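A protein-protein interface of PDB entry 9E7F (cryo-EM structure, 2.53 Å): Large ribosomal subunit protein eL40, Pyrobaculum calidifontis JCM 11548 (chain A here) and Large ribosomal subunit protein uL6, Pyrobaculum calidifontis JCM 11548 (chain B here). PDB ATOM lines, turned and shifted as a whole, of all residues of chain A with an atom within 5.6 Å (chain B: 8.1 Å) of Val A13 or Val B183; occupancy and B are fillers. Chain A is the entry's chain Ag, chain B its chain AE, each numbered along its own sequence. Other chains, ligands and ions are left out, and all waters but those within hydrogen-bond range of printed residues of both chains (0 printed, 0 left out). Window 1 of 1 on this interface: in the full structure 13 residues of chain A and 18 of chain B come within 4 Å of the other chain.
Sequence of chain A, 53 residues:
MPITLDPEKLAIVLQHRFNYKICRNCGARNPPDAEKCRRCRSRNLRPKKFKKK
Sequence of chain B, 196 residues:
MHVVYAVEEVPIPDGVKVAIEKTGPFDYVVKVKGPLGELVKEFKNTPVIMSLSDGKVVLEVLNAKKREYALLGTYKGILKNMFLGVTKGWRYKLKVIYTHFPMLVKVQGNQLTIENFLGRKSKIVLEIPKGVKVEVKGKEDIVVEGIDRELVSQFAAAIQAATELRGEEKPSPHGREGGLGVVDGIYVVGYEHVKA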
ATOM      1  N   ILE A   3      29.556 -25.413   8.536  1.00  0.00           N
ATOM      2  CA  ILE A   3      28.847 -25.332   9.804  1.00  0.00           C
ATOM      3  C   ILE A   3      29.284 -26.482  10.690  1.00  0.00           C
ATOM      4  O   ILE A   3      28.954 -27.635  10.423  1.00  0.00           O
ATOM      5  CB  ILE A   3      27.326 -25.339   9.594  1.00  0.00           C
ATOM      6  CG1 ILE A   3      26.930 -24.262   8.590  1.00  0.00           C
ATOM      7  CG2 ILE A   3      26.605 -25.113  10.906  1.00  0.00           C
ATOM      8  CD1 ILE A   3      25.462 -23.981   8.571  1.00  0.00           C
ATOM      9  N   LEU A   5      30.319 -27.662  14.916  1.00  0.00           N
ATOM     10  CA  LEU A   5      30.354 -27.450  16.352  1.00  0.00           C
ATOM     11  C   LEU A   5      31.401 -28.363  16.977  1.00  0.00           C
ATOM     12  O   LEU A   5      31.874 -29.317  16.355  1.00  0.00           O
ATOM     13  CB  LEU A   5      28.987 -27.727  16.986  1.00  0.00           C
ATOM     14  CG  LEU A   5      27.849 -26.775  16.637  1.00  0.00           C
ATOM     15  CD1 LEU A   5      26.528 -27.368  17.087  1.00  0.00           C
ATOM     16  CD2 LEU A   5      28.078 -25.419  17.269  1.00  0.00           C
ATOM     17  N   LYS A   9      29.069 -29.682  22.101  1.00  0.00           N
ATOM     18  CA  LYS A   9      27.843 -29.143  21.528  1.00  0.00           C
ATOM     19  C   LYS A   9      27.244 -30.088  20.503  1.00  0.00           C
ATOM     20  O   LYS A   9      26.024 -30.106  20.315  1.00  0.00           O
ATOM     21  CB  LYS A   9      28.117 -27.798  20.870  1.00  0.00           C
ATOM     22  CG  LYS A   9      28.271 -26.646  21.820  1.00  0.00           C
ATOM     23  CD  LYS A   9      27.893 -25.365  21.120  1.00  0.00           C
ATOM     24  CE  LYS A   9      29.101 -24.480  20.917  1.00  0.00           C
ATOM     25  NZ  LYS A   9      29.506 -23.815  22.176  1.00  0.00           N
ATOM     26  N   LEU A  10      28.091 -30.858  19.822  1.00  0.00           N
ATOM     27  CA  LEU A  10      27.622 -31.750  18.770  1.00  0.00           C
ATOM     28  C   LEU A  10      26.716 -32.837  19.329  1.00  0.00           C
ATOM     29  O   LEU A  10      25.724 -33.214  18.695  1.00  0.00           O
ATOM     30  CB  LEU A  10      28.818 -32.359  18.049  1.00  0.00           C
ATOM     31  CG  LEU A  10      28.524 -33.510  17.098  1.00  0.00           C
ATOM     32  CD1 LEU A  10      27.634 -33.042  15.968  1.00  0.00           C
ATOM     33  CD2 LEU A  10      29.824 -34.080  16.566  1.00  0.00           C
ATOM     34  N   ALA A  11      27.046 -33.359  20.510  1.00  0.00           N
ATOM     35  CA  ALA A  11      26.173 -34.334  21.151  1.00  0.00           C
ATOM     36  C   ALA A  11      24.840 -33.710  21.535  1.00  0.00           C
ATOM     37  O   ALA A  11      23.787 -34.341  21.398  1.00  0.00           O
ATOM     38  CB  ALA A  11      26.860 -34.922  22.379  1.00  0.00           C
ATOM     39  N   ILE A  12      24.872 -32.468  22.023  1.00  0.00           N
ATOM     40  CA  ILE A  12      23.652 -31.797  22.467  1.00  0.00           C
ATOM     41  C   ILE A  12      22.728 -31.538  21.286  1.00  0.00           C
ATOM     42  O   ILE A  12      21.514 -31.748  21.366  1.00  0.00           O
ATOM     43  CB  ILE A  12      24.002 -30.493  23.201  1.00  0.00           C
ATOM     44  CG1 ILE A  12      24.230 -30.766  24.685  1.00  0.00           C
ATOM     45  CG2 ILE A  12      22.909 -29.465  23.006  1.00  0.00           C
ATOM     46  CD1 ILE A  12      22.965 -30.968  25.466  1.00  0.00           C
ATOM     47  N   VAL A  13      23.295 -31.079  20.172  1.00  0.00           N
ATOM     48  CA  VAL A  13      22.492 -30.767  18.995  1.00  0.00           C
ATOM     49  C   VAL A  13      21.903 -32.035  18.399  1.00  0.00           C
ATOM     50  O   VAL A  13      20.762 -32.042  17.921  1.00  0.00           O
ATOM     51  CB  VAL A  13      23.341 -30.003  17.965  1.00  0.00           C
ATOM     52  CG1 VAL A  13      22.612 -29.922  16.641  1.00  0.00           C
ATOM     53  CG2 VAL A  13      23.681 -28.625  18.481  1.00  0.00           C
ATOM     54  N   LEU A  14      22.668 -33.125  18.409  1.00  0.00           N
ATOM     55  CA  LEU A  14      22.170 -34.376  17.849  1.00  0.00           C
ATOM     56  C   LEU A  14      21.044 -34.958  18.688  1.00  0.00           C
ATOM     57  O   LEU A  14      20.179 -35.664  18.160  1.00  0.00           O
ATOM     58  CB  LEU A  14      23.312 -35.383  17.725  1.00  0.00           C
ATOM     59  CG  LEU A  14      23.783 -35.681  16.304  1.00  0.00           C
ATOM     60  CD1 LEU A  14      24.072 -34.390  15.564  1.00  0.00           C
ATOM     61  CD2 LEU A  14      25.012 -36.558  16.342  1.00  0.00           C
ATOM     62  N   GLN A  15      21.039 -34.686  19.989  1.00  0.00           N
ATOM     63  CA  GLN A  15      20.008 -35.216  20.865  1.00  0.00           C
ATOM     64  C   GLN A  15      18.714 -34.419  20.817  1.00  0.00           C
ATOM     65  O   GLN A  15      17.666 -34.940  21.213  1.00  0.00           O
ATOM     66  CB  GLN A  15      20.516 -35.269  22.310  1.00  0.00           C
ATOM     67  CG  GLN A  15      20.002 -36.420  23.207  1.00  0.00           C
ATOM     68  CD  GLN A  15      20.059 -37.845  22.620  1.00  0.00           C
ATOM     69  OE1 GLN A  15      20.337 -38.069  21.442  1.00  0.00           O
ATOM     70  NE2 GLN A  15      19.785 -38.820  23.475  1.00  0.00           N
ATOM     71  N   HIS A  16      18.761 -33.175  20.350  1.00  0.00           N
ATOM     72  CA  HIS A  16      17.583 -32.326  20.301  1.00  0.00           C
ATOM     73  C   HIS A  16      17.010 -32.175  18.904  1.00  0.00           C
ATOM     74  O   HIS A  16      15.856 -31.758  18.770  1.00  0.00           O
ATOM     75  CB  HIS A  16      17.906 -30.936  20.851  1.00  0.00           C
ATOM     76  CG  HIS A  16      18.005 -30.886  22.341  1.00  0.00           C
ATOM     77  ND1 HIS A  16      16.922 -30.630  23.150  1.00  0.00           N
ATOM     78  CD2 HIS A  16      19.061 -31.060  23.169  1.00  0.00           C
ATOM     79  CE1 HIS A  16      17.305 -30.648  24.413  1.00  0.00           C
ATOM     80  NE2 HIS A  16      18.598 -30.906  24.452  1.00  0.00           N
ATOM     81  N   ARG A  17      17.778 -32.496  17.866  1.00  0.00           N
ATOM     82  CA  ARG A  17      17.327 -32.302  16.501  1.00  0.00           C
ATOM     83  C   ARG A  17      17.362 -33.558  15.645  1.00  0.00           C
ATOM     84  O   ARG A  17      16.773 -33.555  14.559  1.00  0.00           O
ATOM     85  CB  ARG A  17      18.163 -31.211  15.814  1.00  0.00           C
ATOM     86  CG  ARG A  17      18.467 -30.010  16.688  1.00  0.00           C
ATOM     87  CD  ARG A  17      18.123 -28.711  15.981  1.00  0.00           C
ATOM     88  NE  ARG A  17      17.846 -27.630  16.922  1.00  0.00           N
ATOM     89  CZ  ARG A  17      17.534 -26.388  16.570  1.00  0.00           C
ATOM     90  NH1 ARG A  17      17.460 -26.028  15.301  1.00  0.00           N
ATOM     91  NH2 ARG A  17      17.294 -25.487  17.517  1.00  0.00           N
ATOM     92  N   PHE A  18      18.025 -34.629  16.090  1.00  0.00           N
ATOM     93  CA  PHE A  18      18.212 -35.791  15.228  1.00  0.00           C
ATOM     94  C   PHE A  18      17.939 -37.112  15.938  1.00  0.00           C
ATOM     95  O   PHE A  18      18.355 -38.164  15.440  1.00  0.00           O
ATOM     96  CB  PHE A  18      19.633 -35.824  14.660  1.00  0.00           C
ATOM     97  CG  PHE A  18      19.975 -34.645  13.801  1.00  0.00           C
ATOM     98  CD1 PHE A  18      20.487 -33.486  14.359  1.00  0.00           C
ATOM     99  CD2 PHE A  18      19.801 -34.699  12.432  1.00  0.00           C
ATOM    100  CE1 PHE A  18      20.805 -32.406  13.570  1.00  0.00           C
ATOM    101  CE2 PHE A  18      20.123 -33.621  11.639  1.00  0.00           C
ATOM    102  CZ  PHE A  18      20.624 -32.474  12.209  1.00  0.00           C
ATOM    103  N   LYS B  95      22.319 -24.261  27.371  1.00  0.00           N
ATOM    104  CA  LYS B  95      23.518 -23.920  26.623  1.00  0.00           C
ATOM    105  C   LYS B  95      23.126 -23.184  25.352  1.00  0.00           C
ATOM    106  O   LYS B  95      22.241 -23.635  24.620  1.00  0.00           O
ATOM    107  CB  LYS B  95      24.317 -25.175  26.280  1.00  0.00           C
ATOM    108  CG  LYS B  95      25.763 -24.916  25.932  1.00  0.00           C
ATOM    109  CD  LYS B  95      26.462 -26.213  25.597  1.00  0.00           C
ATOM    110  CE  LYS B  95      26.351 -27.199  26.750  1.00  0.00           C
ATOM    111  NZ  LYS B  95      25.716 -28.481  26.334  1.00  0.00           N
ATOM    112  N   VAL B  96      23.783 -22.060  25.092  1.00  0.00           N
ATOM    113  CA  VAL B  96      23.512 -21.252  23.908  1.00  0.00           C
ATOM    114  C   VAL B  96      24.425 -21.716  22.781  1.00  0.00           C
ATOM    115  O   VAL B  96      25.645 -21.794  22.952  1.00  0.00           O
ATOM    116  CB  VAL B  96      23.712 -19.759  24.200  1.00  0.00           C
ATOM    117  CG1 VAL B  96      23.360 -18.937  22.985  1.00  0.00           C
ATOM    118  CG2 VAL B  96      22.867 -19.341  25.384  1.00  0.00           C
ATOM    119  N   ILE B  97      23.837 -22.022  21.629  1.00  0.00           N
ATOM    120  CA  ILE B  97      24.570 -22.543  20.483  1.00  0.00           C
ATOM    121  C   ILE B  97      24.282 -21.663  19.274  1.00  0.00           C
ATOM    122  O   ILE B  97      23.117 -21.387  18.967  1.00  0.00           O
ATOM    123  CB  ILE B  97      24.202 -24.008  20.193  1.00  0.00           C
ATOM    124  CG1 ILE B  97      24.575 -24.891  21.384  1.00  0.00           C
ATOM    125  CG2 ILE B  97      24.901 -24.492  18.943  1.00  0.00           C
ATOM    126  CD1 ILE B  97      24.395 -26.372  21.138  1.00  0.00           C
ATOM    127  N   TYR B  98      25.341 -21.224  18.596  1.00  0.00           N
ATOM    128  CA  TYR B  98      25.213 -20.452  17.369  1.00  0.00           C
ATOM    129  C   TYR B  98      26.328 -20.838  16.409  1.00  0.00           C
ATOM    130  O   TYR B  98      27.316 -21.468  16.792  1.00  0.00           O
ATOM    131  CB  TYR B  98      25.240 -18.941  17.627  1.00  0.00           C
ATOM    132  CG  TYR B  98      26.366 -18.461  18.506  1.00  0.00           C
ATOM    133  CD1 TYR B  98      27.626 -18.205  17.986  1.00  0.00           C
ATOM    134  CD2 TYR B  98      26.166 -18.260  19.860  1.00  0.00           C
ATOM    135  CE1 TYR B  98      28.650 -17.765  18.788  1.00  0.00           C
ATOM    136  CE2 TYR B  98      27.185 -17.820  20.673  1.00  0.00           C
ATOM    137  CZ  TYR B  98      28.424 -17.576  20.131  1.00  0.00           C
ATOM    138  OH  TYR B  98      29.441 -17.135  20.948  1.00  0.00           O
ATOM    139  N   THR B  99      26.157 -20.449  15.150  1.00  0.00           N
ATOM    140  CA  THR B  99      27.122 -20.751  14.099  1.00  0.00           C
ATOM    141  C   THR B  99      27.851 -19.527  13.569  1.00  0.00           C
ATOM    142  O   THR B  99      29.068 -19.575  13.396  1.00  0.00           O
ATOM    143  CB  THR B  99      26.428 -21.470  12.934  1.00  0.00           C
ATOM    144  OG1 THR B  99      25.239 -20.760  12.567  1.00  0.00           O
ATOM    145  CG2 THR B  99      26.055 -22.887  13.332  1.00  0.00           C
ATOM    146  N   HIS B 100      27.148 -18.441  13.292  1.00  0.00           N
ATOM    147  CA  HIS B 100      27.783 -17.226  12.791  1.00  0.00           C
ATOM    148  C   HIS B 100      27.401 -15.983  13.580  1.00  0.00           C
ATOM    149  O   HIS B 100      28.238 -15.097  13.754  1.00  0.00           O
ATOM    150  CB  HIS B 100      27.429 -17.033  11.304  1.00  0.00           C
ATOM    151  CG  HIS B 100      28.339 -16.094  10.574  1.00  0.00           C
ATOM    152  ND1 HIS B 100      28.481 -14.767  10.918  1.00  0.00           N
ATOM    153  CD2 HIS B 100      29.149 -16.291   9.507  1.00  0.00           C
ATOM    154  CE1 HIS B 100      29.343 -14.190  10.101  1.00  0.00           C
ATOM    155  NE2 HIS B 100      29.762 -15.093   9.235  1.00  0.00           N
ATOM    156  N   MET B 103      24.550 -14.818  20.081  1.00  0.00           N
ATOM    157  CA  MET B 103      23.221 -14.556  20.618  1.00  0.00           C
ATOM    158  C   MET B 103      23.373 -13.829  21.947  1.00  0.00           C
ATOM    159  O   MET B 103      23.530 -14.462  22.992  1.00  0.00           O
ATOM    160  CB  MET B 103      22.466 -15.866  20.799  1.00  0.00           C
ATOM    161  CG  MET B 103      21.393 -16.132  19.783  1.00  0.00           C
ATOM    162  SD  MET B 103      21.100 -17.900  19.682  1.00  0.00           S
ATOM    163  CE  MET B 103      20.359 -18.193  21.278  1.00  0.00           C
ATOM    164  N   PHE B 117      19.807 -13.481  17.064  1.00  0.00           N
ATOM    165  CA  PHE B 117      19.516 -14.872  16.743  1.00  0.00           C
ATOM    166  C   PHE B 117      19.404 -15.029  15.233  1.00  0.00           C
ATOM    167  O   PHE B 117      18.426 -14.583  14.627  1.00  0.00           O
ATOM    168  CB  PHE B 117      18.233 -15.340  17.428  1.00  0.00           C
ATOM    169  CG  PHE B 117      17.850 -16.749  17.085  1.00  0.00           C
ATOM    170  CD1 PHE B 117      18.781 -17.764  17.151  1.00  0.00           C
ATOM    171  CD2 PHE B 117      16.567 -17.056  16.688  1.00  0.00           C
ATOM    172  CE1 PHE B 117      18.442 -19.058  16.839  1.00  0.00           C
ATOM    173  CE2 PHE B 117      16.220 -18.351  16.373  1.00  0.00           C
ATOM    174  CZ  PHE B 117      17.161 -19.352  16.448  1.00  0.00           C
ATOM    175  N   LEU B 118      20.420 -15.632  14.621  1.00  0.00           N
ATOM    176  CA  LEU B 118      20.566 -15.759  13.174  1.00  0.00           C
ATOM    177  C   LEU B 118      20.746 -14.416  12.478  1.00  0.00           C
ATOM    178  O   LEU B 118      20.568 -14.330  11.260  1.00  0.00           O
ATOM    179  CB  LEU B 118      19.384 -16.508  12.551  1.00  0.00           C
ATOM    180  CG  LEU B 118      19.014 -17.860  13.159  1.00  0.00           C
ATOM    181  CD1 LEU B 118      17.815 -18.448  12.435  1.00  0.00           C
ATOM    182  CD2 LEU B 118      20.188 -18.812  13.116  1.00  0.00           C
ATOM    183  N   THR B 163      13.941 -20.165  20.364  1.00  0.00           N
ATOM    184  CA  THR B 163      14.958 -20.237  19.328  1.00  0.00           C
ATOM    185  C   THR B 163      14.721 -21.380  18.351  1.00  0.00           C
ATOM    186  O   THR B 163      15.679 -21.886  17.759  1.00  0.00           O
ATOM    187  CB  THR B 163      16.346 -20.367  19.957  1.00  0.00           C
ATOM    188  OG1 THR B 163      16.524 -21.699  20.448  1.00  0.00           O
ATOM    189  CG2 THR B 163      16.496 -19.391  21.104  1.00  0.00           C
ATOM    190  N   GLU B 164      13.475 -21.806  18.177  1.00  0.00           N
ATOM    191  CA  GLU B 164      13.115 -22.850  17.227  1.00  0.00           C
ATOM    192  C   GLU B 164      12.031 -22.304  16.305  1.00  0.00           C
ATOM    193  O   GLU B 164      10.864 -22.215  16.697  1.00  0.00           O
ATOM    194  CB  GLU B 164      12.639 -24.107  17.951  1.00  0.00           C
ATOM    195  CG  GLU B 164      13.515 -25.329  17.763  1.00  0.00           C
ATOM    196  CD  GLU B 164      13.429 -25.912  16.368  1.00  0.00           C
ATOM    197  OE1 GLU B 164      13.592 -25.160  15.385  1.00  0.00           O
ATOM    198  OE2 GLU B 164      13.183 -27.130  16.252  1.00  0.00           O
ATOM    199  N   PRO B 171      14.948 -23.314   9.281  1.00  0.00           N
ATOM    200  CA  PRO B 171      16.102 -23.669   8.452  1.00  0.00           C
ATOM    201  C   PRO B 171      16.300 -25.175   8.385  1.00  0.00           C
ATOM    202  O   PRO B 171      15.782 -25.939   9.201  1.00  0.00           O
ATOM    203  CB  PRO B 171      17.270 -22.996   9.174  1.00  0.00           C
ATOM    204  CG  PRO B 171      16.851 -22.979  10.594  1.00  0.00           C
ATOM    205  CD  PRO B 171      15.351 -22.856  10.620  1.00  0.00           C
ATOM    206  N   SER B 172      17.064 -25.592   7.388  1.00  0.00           N
ATOM    207  CA  SER B 172      17.335 -27.009   7.206  1.00  0.00           C
ATOM    208  C   SER B 172      18.233 -27.514   8.327  1.00  0.00           C
ATOM    209  O   SER B 172      19.247 -26.881   8.635  1.00  0.00           O
ATOM    210  CB  SER B 172      17.988 -27.263   5.856  1.00  0.00           C
ATOM    211  OG  SER B 172      18.440 -28.600   5.759  1.00  0.00           O
ATOM    212  N   PRO B 173      17.899 -28.637   8.964  1.00  0.00           N
ATOM    213  CA  PRO B 173      18.769 -29.151  10.026  1.00  0.00           C
ATOM    214  C   PRO B 173      20.085 -29.704   9.507  1.00  0.00           C
ATOM    215  O   PRO B 173      21.105 -29.589  10.195  1.00  0.00           O
ATOM    216  CB  PRO B 173      17.913 -30.243  10.676  1.00  0.00           C
ATOM    217  CG  PRO B 173      17.035 -30.708   9.582  1.00  0.00           C
ATOM    218  CD  PRO B 173      16.739 -29.510   8.726  1.00  0.00           C
ATOM    219  N   HIS B 174      20.098 -30.295   8.319  1.00  0.00           N
ATOM    220  CA  HIS B 174      21.311 -30.825   7.719  1.00  0.00           C
ATOM    221  C   HIS B 174      21.781 -29.901   6.606  1.00  0.00           C
ATOM    222  O   HIS B 174      20.975 -29.308   5.886  1.00  0.00           O
ATOM    223  CB  HIS B 174      21.089 -32.237   7.172  1.00  0.00           C
ATOM    224  CG  HIS B 174      20.143 -32.297   6.013  1.00  0.00           C
ATOM    225  ND1 HIS B 174      20.548 -32.125   4.707  1.00  0.00           N
ATOM    226  CD2 HIS B 174      18.808 -32.512   5.965  1.00  0.00           C
ATOM    227  CE1 HIS B 174      19.503 -32.228   3.906  1.00  0.00           C
ATOM    228  NE2 HIS B 174      18.435 -32.465   4.644  1.00  0.00           N
ATOM    229  N   GLY B 175      23.093 -29.785   6.474  1.00  0.00           N
ATOM    230  CA  GLY B 175      23.688 -28.906   5.493  1.00  0.00           C
ATOM    231  C   GLY B 175      23.710 -29.526   4.113  1.00  0.00           C
ATOM    232  O   GLY B 175      22.998 -30.488   3.816  1.00  0.00           O
ATOM    233  N   GLY B 179      25.758 -32.737   5.692  1.00  0.00           N
ATOM    234  CA  GLY B 179      26.466 -32.128   6.794  1.00  0.00           C
ATOM    235  C   GLY B 179      25.509 -31.491   7.781  1.00  0.00           C
ATOM    236  O   GLY B 179      24.291 -31.462   7.598  1.00  0.00           O
ATOM    237  N   LEU B 180      26.080 -30.974   8.863  1.00  0.00           N
ATOM    238  CA  LEU B 180      25.277 -30.257   9.840  1.00  0.00           C
ATOM    239  C   LEU B 180      24.763 -28.957   9.234  1.00  0.00           C
ATOM    240  O   LEU B 180      25.530 -28.183   8.657  1.00  0.00           O
ATOM    241  CB  LEU B 180      26.098 -29.973  11.093  1.00  0.00           C
ATOM    242  CG  LEU B 180      25.300 -29.757  12.376  1.00  0.00           C
ATOM    243  CD1 LEU B 180      25.074 -31.079  13.089  1.00  0.00           C
ATOM    244  CD2 LEU B 180      25.994 -28.762  13.285  1.00  0.00           C
ATOM    245  N   GLY B 181      23.462 -28.717   9.364  1.00  0.00           N
ATOM    246  CA  GLY B 181      22.850 -27.510   8.848  1.00  0.00           C
ATOM    247  C   GLY B 181      22.983 -26.359   9.820  1.00  0.00           C
ATOM    248  O   GLY B 181      23.836 -26.352  10.710  1.00  0.00           O
ATOM    249  N   VAL B 182      22.123 -25.362   9.643  1.00  0.00           N
ATOM    250  CA  VAL B 182      22.136 -24.199  10.521  1.00  0.00           C
ATOM    251  C   VAL B 182      21.351 -24.523  11.784  1.00  0.00           C
ATOM    252  O   VAL B 182      20.127 -24.363  11.826  1.00  0.00           O
ATOM    253  CB  VAL B 182      21.565 -22.960   9.812  1.00  0.00           C
ATOM    254  CG1 VAL B 182      21.369 -21.827  10.798  1.00  0.00           C
ATOM    255  CG2 VAL B 182      22.483 -22.532   8.689  1.00  0.00           C
ATOM    256  N   VAL B 183      22.044 -24.996  12.816  1.00  0.00           N
ATOM    257  CA  VAL B 183      21.389 -25.339  14.073  1.00  0.00           C
ATOM    258  C   VAL B 183      21.890 -24.418  15.174  1.00  0.00           C
ATOM    259  O   VAL B 183      22.868 -24.723  15.864  1.00  0.00           O
ATOM    260  CB  VAL B 183      21.620 -26.814  14.437  1.00  0.00           C
ATOM    261  CG1 VAL B 183      20.684 -27.699  13.639  1.00  0.00           C
ATOM    262  CG2 VAL B 183      23.059 -27.199  14.175  1.00  0.00           C
ATOM    263  N   ASP B 184      21.212 -23.295  15.353  1.00  0.00           N
ATOM    264  CA  ASP B 184      21.539 -22.319  16.376  1.00  0.00           C
ATOM    265  C   ASP B 184      20.354 -22.212  17.320  1.00  0.00           C
ATOM    266  O   ASP B 184      19.201 -22.258  16.882  1.00  0.00           O
ATOM    267  CB  ASP B 184      21.836 -20.953  15.756  1.00  0.00           C
ATOM    268  CG  ASP B 184      22.944 -21.002  14.726  1.00  0.00           C
ATOM    269  OD1 ASP B 184      22.923 -21.902  13.866  1.00  0.00           O
ATOM    270  OD2 ASP B 184      23.814 -20.111  14.740  1.00  0.00           O
ATOM    271  N   GLY B 185      20.624 -22.079  18.607  1.00  0.00           N
ATOM    272  CA  GLY B 185      19.545 -21.904  19.555  1.00  0.00           C
ATOM    273  C   GLY B 185      20.005 -22.151  20.976  1.00  0.00           C
ATOM    274  O   GLY B 185      21.195 -22.249  21.260  1.00  0.00           O
ATOM    275  N   ILE B 186      19.018 -22.236  21.860  1.00  0.00           N
ATOM    276  CA  ILE B 186      19.227 -22.490  23.277  1.00  0.00           C
ATOM    277  C   ILE B 186      18.581 -23.822  23.609  1.00  0.00           C
ATOM    278  O   ILE B 186      17.395 -24.027  23.332  1.00  0.00           O
ATOM    279  CB  ILE B 186      18.645 -21.365  24.146  1.00  0.00           C
ATOM    280  CG1 ILE B 186      19.360 -20.052  23.839  1.00  0.00           C
ATOM    281  CG2 ILE B 186      18.768 -21.716  25.608  1.00  0.00           C
ATOM    282  CD1 ILE B 186      18.767 -18.850  24.515  1.00  0.00           C
ATOM    283  N   TYR B 187      19.359 -24.721  24.199  1.00  0.00           N
ATOM    284  CA  TYR B 187      18.931 -26.085  24.461  1.00  0.00           C
ATOM    285  C   TYR B 187      19.026 -26.372  25.951  1.00  0.00           C
ATOM    286  O   TYR B 187      20.004 -25.997  26.601  1.00  0.00           O
ATOM    287  CB  TYR B 187      19.783 -27.100  23.687  1.00  0.00           C
ATOM    288  CG  TYR B 187      19.941 -26.836  22.204  1.00  0.00           C
ATOM    289  CD1 TYR B 187      20.903 -25.958  21.729  1.00  0.00           C
ATOM    290  CD2 TYR B 187      19.155 -27.496  21.279  1.00  0.00           C
ATOM    291  CE1 TYR B 187      21.054 -25.724  20.387  1.00  0.00           C
ATOM    292  CE2 TYR B 187      19.303 -27.273  19.930  1.00  0.00           C
ATOM    293  CZ  TYR B 187      20.256 -26.385  19.491  1.00  0.00           C
ATOM    294  OH  TYR B 187      20.411 -26.156  18.146  1.00  0.00           O
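The side-chain hydroxyl (OH) of Tyr B187 lies within hydrogen-bond range of the guanidinium group (NE) of Arg A17 (3.2 Å). The guanidinium group (NH1) of Arg A17 lies within salt-bridge range of the side-chain carboxylate (OE1) of Glu B164, at 3.97 Å.
The backbone NH of Gly B185 is in hydrogen-bond range of the backbone carbonyl oxygen of Ile B97 (2.6 Å). The backbone NH of Thr B99 sits at hydrogen-bond distance from the side-chain carboxylate of Asp B184 (2.4 Å). O of Tyr B187 sits at hydrogen-bond distance from N of Lys B95 (3.0 Å). The backbone carbonyl oxygen (O) of Ser B172 is in hydrogen-bond range of the backbone NH (N) of Val B182. The backbone NH of Gly B181 sits at hydrogen-bond distance from the backbone carbonyl oxygen of Pro B173 (2.6 Å). The side-chain hydroxyl (OG1) of Thr B163 lies within hydrogen-bond range of the backbone NH (N) of Ile B186 (2.9 Å).
Among the printed residues, merely in contact across the chains: Ile A3 with Gly B181 (3.0 Å), Ile A12 with Lys B95 (3.2 Å), Ile A3 with Val B182 (3.3 Å), Ile A3 with Thr B99 (3.3 Å), Lys A9 with Ile B97 (3.4 Å), Ile A3 with Leu B180 (3.5 Å), Phe A18 with Pro B173 (3.6 Å), Val A13 with Ile B97 (3.6 Å), Arg A17 with Val B183 (3.6 Å), His A16 with Tyr B187 (3.7 Å), Val A13 with Val B183 (3.7 Å), Leu A5 with Ile B97 (3.7 Å), Arg A17 with Asp B184 (3.8 Å), Ile A12 with Ile B97 (3.9 Å), Arg A17 with Thr B163 (3.95 Å) and Ile A12 with Tyr B187 (3.98 Å).
Of the printed residues of chain B, Ile A3 touches Thr B99, Leu B180, Gly B181 and Val B182. Printed residues of chain B within 4 Å of Ile A12: Lys B95 (3.2 Å), Ile B97 (3.9 Å) and Tyr B187 (3.98 Å). Of the printed residues of chain B, His A16 touches Tyr B187. Of the printed residues of chain A, Ile B97 touches Leu A5, Lys A9, Ile A12 and Val A13. His B100 touches none of the printed residues of chain A. Leu B118 touches none of the printed residues of chain A. Of the printed residues of chain A, Val B183 touches Val A13 and Arg A17. The nearest residue of chain A that does not touch Val B183 is Leu A5 (4.5 Å). The nearest printed residue of chain B that does not touch Ile A12 is Ile B186 (7.1 Å).
Of the 25 printed residues of chain B, 12 touch a printed residue of chain A. Hydrophobic or aromatic side chains of chain B that line the printed part of chain A: Ile B97, Pro B173, Leu B180, Val B182, Val B183 and Tyr B187. Of the 12 printed residues of chain A, 8 touch a printed residue of chain B. Hydrophobic or aromatic side chains of chain A within 4 Å of the printed part of chain B: Ile A3, Leu A5, Ile A12, Val A13, His A16 and Phe A18. Among the printed residues, Asp or Glu carboxylates within 4 Å of a Lys or Arg side-chain nitrogen of the other chain: Arg A17 with Glu B164.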
